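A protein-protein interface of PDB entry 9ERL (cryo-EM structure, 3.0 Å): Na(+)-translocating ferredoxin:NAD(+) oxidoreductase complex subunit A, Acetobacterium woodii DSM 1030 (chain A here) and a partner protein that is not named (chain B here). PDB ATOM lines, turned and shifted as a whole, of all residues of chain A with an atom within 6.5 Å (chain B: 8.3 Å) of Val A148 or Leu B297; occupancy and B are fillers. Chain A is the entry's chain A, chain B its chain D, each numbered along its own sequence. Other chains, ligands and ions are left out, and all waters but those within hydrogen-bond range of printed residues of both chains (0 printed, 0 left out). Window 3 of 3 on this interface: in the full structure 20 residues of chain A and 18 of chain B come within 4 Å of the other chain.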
ATOM      1  N   PHE A  27      31.133  18.816 -23.854  1.00  0.00           N
ATOM      2  CA  PHE A  27      31.076  17.429 -23.407  1.00  0.00           C
ATOM      3  C   PHE A  27      30.128  17.276 -22.226  1.00  0.00           C
ATOM      4  O   PHE A  27      29.362  16.309 -22.155  1.00  0.00           O
ATOM      5  CB  PHE A  27      32.481  16.953 -23.037  1.00  0.00           C
ATOM      6  CG  PHE A  27      32.621  15.467 -22.914  1.00  0.00           C
ATOM      7  CD1 PHE A  27      32.338  14.637 -23.981  1.00  0.00           C
ATOM      8  CD2 PHE A  27      33.067  14.901 -21.731  1.00  0.00           C
ATOM      9  CE1 PHE A  27      32.481  13.270 -23.865  1.00  0.00           C
ATOM     10  CE2 PHE A  27      33.210  13.537 -21.611  1.00  0.00           C
ATOM     11  CZ  PHE A  27      32.917  12.721 -22.678  1.00  0.00           C
ATOM     12  N   VAL A  34      21.198  11.090 -26.902  1.00  0.00           N
ATOM     13  CA  VAL A  34      22.002  10.555 -28.000  1.00  0.00           C
ATOM     14  C   VAL A  34      21.871  11.368 -29.282  1.00  0.00           C
ATOM     15  O   VAL A  34      22.883  11.596 -29.964  1.00  0.00           O
ATOM     16  CB  VAL A  34      21.630   9.078 -28.254  1.00  0.00           C
ATOM     17  CG1 VAL A  34      22.321   8.539 -29.496  1.00  0.00           C
ATOM     18  CG2 VAL A  34      21.989   8.233 -27.046  1.00  0.00           C
ATOM     19  N   ALA A  37      23.823  14.660 -29.197  1.00  0.00           N
ATOM     20  CA  ALA A  37      25.247  14.362 -29.298  1.00  0.00           C
ATOM     21  C   ALA A  37      25.659  14.099 -30.741  1.00  0.00           C
ATOM     22  O   ALA A  37      26.700  14.587 -31.194  1.00  0.00           O
ATOM     23  CB  ALA A  37      25.591  13.165 -28.413  1.00  0.00           C
ATOM     24  N   VAL A  38      24.845  13.342 -31.482  1.00  0.00           N
ATOM     25  CA  VAL A  38      25.152  13.048 -32.879  1.00  0.00           C
ATOM     26  C   VAL A  38      25.116  14.320 -33.720  1.00  0.00           C
ATOM     27  O   VAL A  38      25.988  14.544 -34.574  1.00  0.00           O
ATOM     28  CB  VAL A  38      24.182  11.978 -33.415  1.00  0.00           C
ATOM     29  CG1 VAL A  38      24.292  11.852 -34.925  1.00  0.00           C
ATOM     30  CG2 VAL A  38      24.448  10.643 -32.744  1.00  0.00           C
ATOM     31  N   PHE A 143      36.073  13.041 -31.024  1.00  0.00           N
ATOM     32  CA  PHE A 143      35.129  13.829 -30.234  1.00  0.00           C
ATOM     33  C   PHE A 143      33.723  13.239 -30.301  1.00  0.00           C
ATOM     34  O   PHE A 143      33.037  13.122 -29.273  1.00  0.00           O
ATOM     35  CB  PHE A 143      35.132  15.280 -30.723  1.00  0.00           C
ATOM     36  CG  PHE A 143      34.146  16.174 -30.016  1.00  0.00           C
ATOM     37  CD1 PHE A 143      34.455  16.736 -28.789  1.00  0.00           C
ATOM     38  CD2 PHE A 143      32.920  16.469 -30.590  1.00  0.00           C
ATOM     39  CE1 PHE A 143      33.555  17.561 -28.141  1.00  0.00           C
ATOM     40  CE2 PHE A 143      32.017  17.292 -29.945  1.00  0.00           C
ATOM     41  CZ  PHE A 143      32.336  17.839 -28.719  1.00  0.00           C
ATOM     42  N   THR A 144      33.284  12.852 -31.504  1.00  0.00           N
ATOM     43  CA  THR A 144      31.948  12.283 -31.666  1.00  0.00           C
ATOM     44  C   THR A 144      31.798  10.975 -30.897  1.00  0.00           C
ATOM     45  O   THR A 144      30.784  10.756 -30.221  1.00  0.00           O
ATOM     46  CB  THR A 144      31.649  12.060 -33.148  1.00  0.00           C
ATOM     47  OG1 THR A 144      32.167  13.155 -33.912  1.00  0.00           O
ATOM     48  CG2 THR A 144      30.151  11.951 -33.376  1.00  0.00           C
ATOM     49  N   LEU A 145      32.803  10.096 -30.981  1.00  0.00           N
ATOM     50  CA  LEU A 145      32.736   8.826 -30.267  1.00  0.00           C
ATOM     51  C   LEU A 145      32.676   9.040 -28.759  1.00  0.00           C
ATOM     52  O   LEU A 145      31.872   8.401 -28.063  1.00  0.00           O
ATOM     53  CB  LEU A 145      33.937   7.955 -30.639  1.00  0.00           C
ATOM     54  CG  LEU A 145      34.016   6.564 -30.009  1.00  0.00           C
ATOM     55  CD1 LEU A 145      33.105   5.588 -30.733  1.00  0.00           C
ATOM     56  CD2 LEU A 145      35.451   6.059 -30.003  1.00  0.00           C
ATOM     57  N   ALA A 146      33.505   9.954 -28.240  1.00  0.00           N
ATOM     58  CA  ALA A 146      33.508  10.210 -26.803  1.00  0.00           C
ATOM     59  C   ALA A 146      32.165  10.751 -26.326  1.00  0.00           C
ATOM     60  O   ALA A 146      31.629  10.293 -25.306  1.00  0.00           O
ATOM     61  CB  ALA A 146      34.633  11.179 -26.444  1.00  0.00           C
ATOM     62  N   ILE A 147      31.591  11.712 -27.059  1.00  0.00           N
ATOM     63  CA  ILE A 147      30.332  12.297 -26.600  1.00  0.00           C
ATOM     64  C   ILE A 147      29.183  11.294 -26.713  1.00  0.00           C
ATOM     65  O   ILE A 147      28.286  11.279 -25.858  1.00  0.00           O
ATOM     66  CB  ILE A 147      30.040  13.624 -27.334  1.00  0.00           C
ATOM     67  CG1 ILE A 147      28.966  14.418 -26.589  1.00  0.00           C
ATOM     68  CG2 ILE A 147      29.640  13.408 -28.786  1.00  0.00           C
ATOM     69  CD1 ILE A 147      28.885  15.869 -26.996  1.00  0.00           C
ATOM     70  N   VAL A 148      29.200  10.419 -27.726  1.00  0.00           N
ATOM     71  CA  VAL A 148      28.142   9.417 -27.846  1.00  0.00           C
ATOM     72  C   VAL A 148      28.217   8.407 -26.704  1.00  0.00           C
ATOM     73  O   VAL A 148      27.190   8.042 -26.108  1.00  0.00           O
ATOM     74  CB  VAL A 148      28.213   8.736 -29.226  1.00  0.00           C
ATOM     75  CG1 VAL A 148      27.439   7.430 -29.226  1.00  0.00           C
ATOM     76  CG2 VAL A 148      27.673   9.666 -30.299  1.00  0.00           C
ATOM     77  N   LEU A 149      29.430   7.951 -26.366  1.00  0.00           N
ATOM     78  CA  LEU A 149      29.576   7.022 -25.247  1.00  0.00           C
ATOM     79  C   LEU A 149      29.143   7.663 -23.930  1.00  0.00           C
ATOM     80  O   LEU A 149      28.482   7.018 -23.102  1.00  0.00           O
ATOM     81  CB  LEU A 149      31.020   6.528 -25.155  1.00  0.00           C
ATOM     82  CG  LEU A 149      31.530   5.639 -26.293  1.00  0.00           C
ATOM     83  CD1 LEU A 149      32.985   5.272 -26.068  1.00  0.00           C
ATOM     84  CD2 LEU A 149      30.681   4.391 -26.442  1.00  0.00           C
ATOM     85  N   PHE A 150      29.497   8.937 -23.724  1.00  0.00           N
ATOM     86  CA  PHE A 150      29.079   9.638 -22.512  1.00  0.00           C
ATOM     87  C   PHE A 150      27.562   9.752 -22.423  1.00  0.00           C
ATOM     88  O   PHE A 150      26.978   9.553 -21.348  1.00  0.00           O
ATOM     89  CB  PHE A 150      29.721  11.024 -22.467  1.00  0.00           C
ATOM     90  CG  PHE A 150      29.761  11.632 -21.095  1.00  0.00           C
ATOM     91  CD1 PHE A 150      29.857  10.833 -19.970  1.00  0.00           C
ATOM     92  CD2 PHE A 150      29.699  13.004 -20.933  1.00  0.00           C
ATOM     93  CE1 PHE A 150      29.894  11.394 -18.711  1.00  0.00           C
ATOM     94  CE2 PHE A 150      29.736  13.569 -19.676  1.00  0.00           C
ATOM     95  CZ  PHE A 150      29.833  12.763 -18.564  1.00  0.00           C
ATOM     96  N   ALA A 151      26.906  10.078 -23.542  1.00  0.00           N
ATOM     97  CA  ALA A 151      25.449  10.188 -23.543  1.00  0.00           C
ATOM     98  C   ALA A 151      24.791   8.851 -23.225  1.00  0.00           C
ATOM     99  O   ALA A 151      23.809   8.797 -22.471  1.00  0.00           O
ATOM    100  CB  ALA A 151      24.966  10.718 -24.891  1.00  0.00           C
ATOM    101  N   GLY A 152      25.322   7.761 -23.785  1.00  0.00           N
ATOM    102  CA  GLY A 152      24.782   6.446 -23.467  1.00  0.00           C
ATOM    103  C   GLY A 152      24.931   6.085 -22.000  1.00  0.00           C
ATOM    104  O   GLY A 152      24.007   5.542 -21.384  1.00  0.00           O
ATOM    105  N   ILE A 153      26.093   6.394 -21.415  1.00  0.00           N
ATOM    106  CA  ILE A 153      26.310   6.090 -20.000  1.00  0.00           C
ATOM    107  C   ILE A 153      25.367   6.905 -19.121  1.00  0.00           C
ATOM    108  O   ILE A 153      24.827   6.398 -18.130  1.00  0.00           O
ATOM    109  CB  ILE A 153      27.785   6.317 -19.618  1.00  0.00           C
ATOM    110  CG1 ILE A 153      28.678   5.273 -20.287  1.00  0.00           C
ATOM    111  CG2 ILE A 153      27.970   6.248 -18.118  1.00  0.00           C
ATOM    112  CD1 ILE A 153      30.110   5.711 -20.431  1.00  0.00           C
ATOM    113  N   PRO B 254      25.913  -7.104 -20.385  1.00  0.00           N
ATOM    114  CA  PRO B 254      24.580  -7.016 -20.994  1.00  0.00           C
ATOM    115  C   PRO B 254      23.666  -8.133 -20.515  1.00  0.00           C
ATOM    116  O   PRO B 254      24.107  -9.189 -20.059  1.00  0.00           O
ATOM    117  CB  PRO B 254      24.865  -7.135 -22.496  1.00  0.00           C
ATOM    118  CG  PRO B 254      26.313  -6.806 -22.643  1.00  0.00           C
ATOM    119  CD  PRO B 254      26.957  -7.318 -21.400  1.00  0.00           C
ATOM    120  N   ILE B 262      28.854 -10.231 -28.556  1.00  0.00           N
ATOM    121  CA  ILE B 262      29.627  -9.093 -29.058  1.00  0.00           C
ATOM    122  C   ILE B 262      30.610  -8.598 -27.999  1.00  0.00           C
ATOM    123  O   ILE B 262      31.762  -8.255 -28.308  1.00  0.00           O
ATOM    124  CB  ILE B 262      28.678  -7.977 -29.528  1.00  0.00           C
ATOM    125  CG1 ILE B 262      27.785  -8.483 -30.661  1.00  0.00           C
ATOM    126  CG2 ILE B 262      29.457  -6.754 -29.979  1.00  0.00           C
ATOM    127  CD1 ILE B 262      26.521  -7.683 -30.847  1.00  0.00           C
ATOM    128  N   MET B 291      35.141  -2.345 -22.373  1.00  0.00           N
ATOM    129  CA  MET B 291      33.866  -2.911 -22.785  1.00  0.00           C
ATOM    130  C   MET B 291      32.761  -2.684 -21.764  1.00  0.00           C
ATOM    131  O   MET B 291      31.602  -3.003 -22.044  1.00  0.00           O
ATOM    132  CB  MET B 291      34.019  -4.407 -23.065  1.00  0.00           C
ATOM    133  CG  MET B 291      34.687  -4.712 -24.393  1.00  0.00           C
ATOM    134  SD  MET B 291      33.569  -4.515 -25.791  1.00  0.00           S
ATOM    135  CE  MET B 291      34.570  -3.513 -26.884  1.00  0.00           C
ATOM    136  N   ASN B 292      33.090  -2.155 -20.586  1.00  0.00           N
ATOM    137  CA  ASN B 292      32.091  -1.663 -19.648  1.00  0.00           C
ATOM    138  C   ASN B 292      31.573  -0.284 -20.024  1.00  0.00           C
ATOM    139  O   ASN B 292      30.520   0.125 -19.528  1.00  0.00           O
ATOM    140  CB  ASN B 292      32.672  -1.612 -18.229  1.00  0.00           C
ATOM    141  CG  ASN B 292      32.903  -2.986 -17.645  1.00  0.00           C
ATOM    142  OD1 ASN B 292      32.458  -3.990 -18.195  1.00  0.00           O
ATOM    143  ND2 ASN B 292      33.604  -3.039 -16.522  1.00  0.00           N
ATOM    144  N   VAL B 293      32.288   0.433 -20.888  1.00  0.00           N
ATOM    145  CA  VAL B 293      31.850   1.740 -21.353  1.00  0.00           C
ATOM    146  C   VAL B 293      30.923   1.617 -22.560  1.00  0.00           C
ATOM    147  O   VAL B 293      29.922   2.337 -22.650  1.00  0.00           O
ATOM    148  CB  VAL B 293      33.081   2.612 -21.667  1.00  0.00           C
ATOM    149  CG1 VAL B 293      32.698   3.855 -22.452  1.00  0.00           C
ATOM    150  CG2 VAL B 293      33.806   2.989 -20.384  1.00  0.00           C
ATOM    151  N   ALA B 294      31.217   0.699 -23.478  1.00  0.00           N
ATOM    152  CA  ALA B 294      30.418   0.503 -24.679  1.00  0.00           C
ATOM    153  C   ALA B 294      29.201  -0.386 -24.459  1.00  0.00           C
ATOM    154  O   ALA B 294      28.428  -0.584 -25.401  1.00  0.00           O
ATOM    155  CB  ALA B 294      31.282  -0.094 -25.792  1.00  0.00           C
ATOM    156  N   THR B 295      29.022  -0.931 -23.254  1.00  0.00           N
ATOM    157  CA  THR B 295      27.883  -1.811 -22.989  1.00  0.00           C
ATOM    158  C   THR B 295      26.527  -1.124 -23.152  1.00  0.00           C
ATOM    159  O   THR B 295      25.632  -1.735 -23.763  1.00  0.00           O
ATOM    160  CB  THR B 295      28.042  -2.453 -21.605  1.00  0.00           C
ATOM    161  OG1 THR B 295      29.132  -3.381 -21.632  1.00  0.00           O
ATOM    162  CG2 THR B 295      26.781  -3.188 -21.197  1.00  0.00           C
ATOM    163  N   PRO B 296      26.289   0.103 -22.654  1.00  0.00           N
ATOM    164  CA  PRO B 296      24.984   0.738 -22.921  1.00  0.00           C
ATOM    165  C   PRO B 296      24.691   0.974 -24.395  1.00  0.00           C
ATOM    166  O   PRO B 296      23.516   1.083 -24.770  1.00  0.00           O
ATOM    167  CB  PRO B 296      25.084   2.061 -22.153  1.00  0.00           C
ATOM    168  CG  PRO B 296      25.992   1.759 -21.041  1.00  0.00           C
ATOM    169  CD  PRO B 296      27.043   0.890 -21.656  1.00  0.00           C
ATOM    170  N   LEU B 297      25.714   1.068 -25.242  1.00  0.00           N
ATOM    171  CA  LEU B 297      25.503   1.202 -26.678  1.00  0.00           C
ATOM    172  C   LEU B 297      25.140  -0.115 -27.349  1.00  0.00           C
ATOM    173  O   LEU B 297      24.351  -0.117 -28.300  1.00  0.00           O
ATOM    174  CB  LEU B 297      26.752   1.787 -27.342  1.00  0.00           C
ATOM    175  CG  LEU B 297      26.528   3.036 -28.194  1.00  0.00           C
ATOM    176  CD1 LEU B 297      25.952   4.160 -27.347  1.00  0.00           C
ATOM    177  CD2 LEU B 297      27.820   3.472 -28.858  1.00  0.00           C
ATOM    178  N   ILE B 298      25.704  -1.234 -26.887  1.00  0.00           N
ATOM    179  CA  ILE B 298      25.322  -2.538 -27.417  1.00  0.00           C
ATOM    180  C   ILE B 298      23.894  -2.899 -27.033  1.00  0.00           C
ATOM    181  O   ILE B 298      23.177  -3.514 -27.830  1.00  0.00           O
ATOM    182  CB  ILE B 298      26.299  -3.631 -26.939  1.00  0.00           C
ATOM    183  CG1 ILE B 298      27.748  -3.207 -27.178  1.00  0.00           C
ATOM    184  CG2 ILE B 298      26.028  -4.949 -27.644  1.00  0.00           C
ATOM    185  CD1 ILE B 298      28.763  -4.169 -26.609  1.00  0.00           C
ATOM    186  N   GLU B 299      23.458  -2.521 -25.833  1.00  0.00           N
ATOM    187  CA  GLU B 299      22.157  -2.924 -25.318  1.00  0.00           C
ATOM    188  C   GLU B 299      20.985  -2.256 -26.024  1.00  0.00           C
ATOM    189  O   GLU B 299      19.857  -2.748 -25.913  1.00  0.00           O
ATOM    190  CB  GLU B 299      22.080  -2.628 -23.818  1.00  0.00           C
ATOM    191  CG  GLU B 299      22.772  -3.665 -22.955  1.00  0.00           C
ATOM    192  CD  GLU B 299      22.322  -3.620 -21.512  1.00  0.00           C
ATOM    193  OE1 GLU B 299      22.786  -2.730 -20.770  1.00  0.00           O
ATOM    194  OE2 GLU B 299      21.503  -4.474 -21.118  1.00  0.00           O
ATOM    195  N   ARG B 300      21.212  -1.157 -26.740  1.00  0.00           N
ATOM    196  CA  ARG B 300      20.140  -0.467 -27.446  1.00  0.00           C
ATOM    197  C   ARG B 300      19.958  -0.952 -28.878  1.00  0.00           C
ATOM    198  O   ARG B 300      19.030  -0.500 -29.554  1.00  0.00           O
ATOM    199  CB  ARG B 300      20.390   1.044 -27.444  1.00  0.00           C
ATOM    200  CG  ARG B 300      21.483   1.492 -28.394  1.00  0.00           C
ATOM    201  CD  ARG B 300      21.513   3.004 -28.544  1.00  0.00           C
ATOM    202  NE  ARG B 300      20.265   3.541 -29.071  1.00  0.00           N
ATOM    203  CZ  ARG B 300      19.569   4.514 -28.500  1.00  0.00           C
ATOM    204  NH1 ARG B 300      19.958   5.067 -27.363  1.00  0.00           N
ATOM    205  NH2 ARG B 300      18.454   4.943 -29.083  1.00  0.00           N
ATOM    206  N   PHE B 301      20.813  -1.859 -29.353  1.00  0.00           N
ATOM    207  CA  PHE B 301      20.692  -2.403 -30.697  1.00  0.00           C
ATOM    208  C   PHE B 301      20.463  -3.906 -30.728  1.00  0.00           C
ATOM    209  O   PHE B 301      20.322  -4.467 -31.819  1.00  0.00           O
ATOM    210  CB  PHE B 301      21.945  -2.080 -31.528  1.00  0.00           C
ATOM    211  CG  PHE B 301      22.104  -0.624 -31.854  1.00  0.00           C
ATOM    212  CD1 PHE B 301      21.059   0.096 -32.404  1.00  0.00           C
ATOM    213  CD2 PHE B 301      23.305   0.023 -31.618  1.00  0.00           C
ATOM    214  CE1 PHE B 301      21.205   1.437 -32.708  1.00  0.00           C
ATOM    215  CE2 PHE B 301      23.459   1.361 -31.919  1.00  0.00           C
ATOM    216  CZ  PHE B 301      22.407   2.069 -32.464  1.00  0.00           C
ATOM    217  N   THR B 302      20.422  -4.573 -29.578  1.00  0.00           N
ATOM    218  CA  THR B 302      20.298  -6.025 -29.516  1.00  0.00           C
ATOM    219  C   THR B 302      19.100  -6.434 -28.673  1.00  0.00           C
ATOM    220  O   THR B 302      19.151  -7.410 -27.920  1.00  0.00           O
ATOM    221  CB  THR B 302      21.573  -6.663 -28.968  1.00  0.00           C
ATOM    222  OG1 THR B 302      21.881  -6.095 -27.690  1.00  0.00           O
ATOM    223  CG2 THR B 302      22.740  -6.430 -29.916  1.00  0.00           C
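CG2 of Val A34 touches NH1 of Arg B300, at 3.8 Å.
Leu B297 touches Val A148 (CD2 to CG1, 3.99 Å).
Val B293 touches Leu A149 (CG1 to CD1, 3.9 Å).
Leu B297 touches Leu A149.
O of Gly A152 touches CB of Pro B296, at 3.7 Å.
Ile A153 touches Val B293.
Printed residues of chain B within 4 Å of Val A148: Leu B297.
Of the printed residues of chain B, Leu A149 touches Val B293 and Leu B297.
Of the printed residues of chain B, Gly A152 touches Pro B296 (3.7 Å).
Printed residues of chain A within 4 Å of Pro B296: Gly A152.
Thr B302 touches none of the printed residues of chain A.
The nearest printed residue of chain B that does not touch Val A148 is Val B293 (7.2 Å).
The nearest printed residue of chain A that does not touch Leu B297 is Gly A152 (4.7 Å).
The nearest printed residue of chain B that does not touch Ile A153 is Pro B296 (4.5 Å).
Of the 15 printed residues of chain A, 5 touch a printed residue of chain B.
Hydrophobic or aromatic side chains of chain B that line the printed part of chain A: Val B293, Pro B296 and Leu B297.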
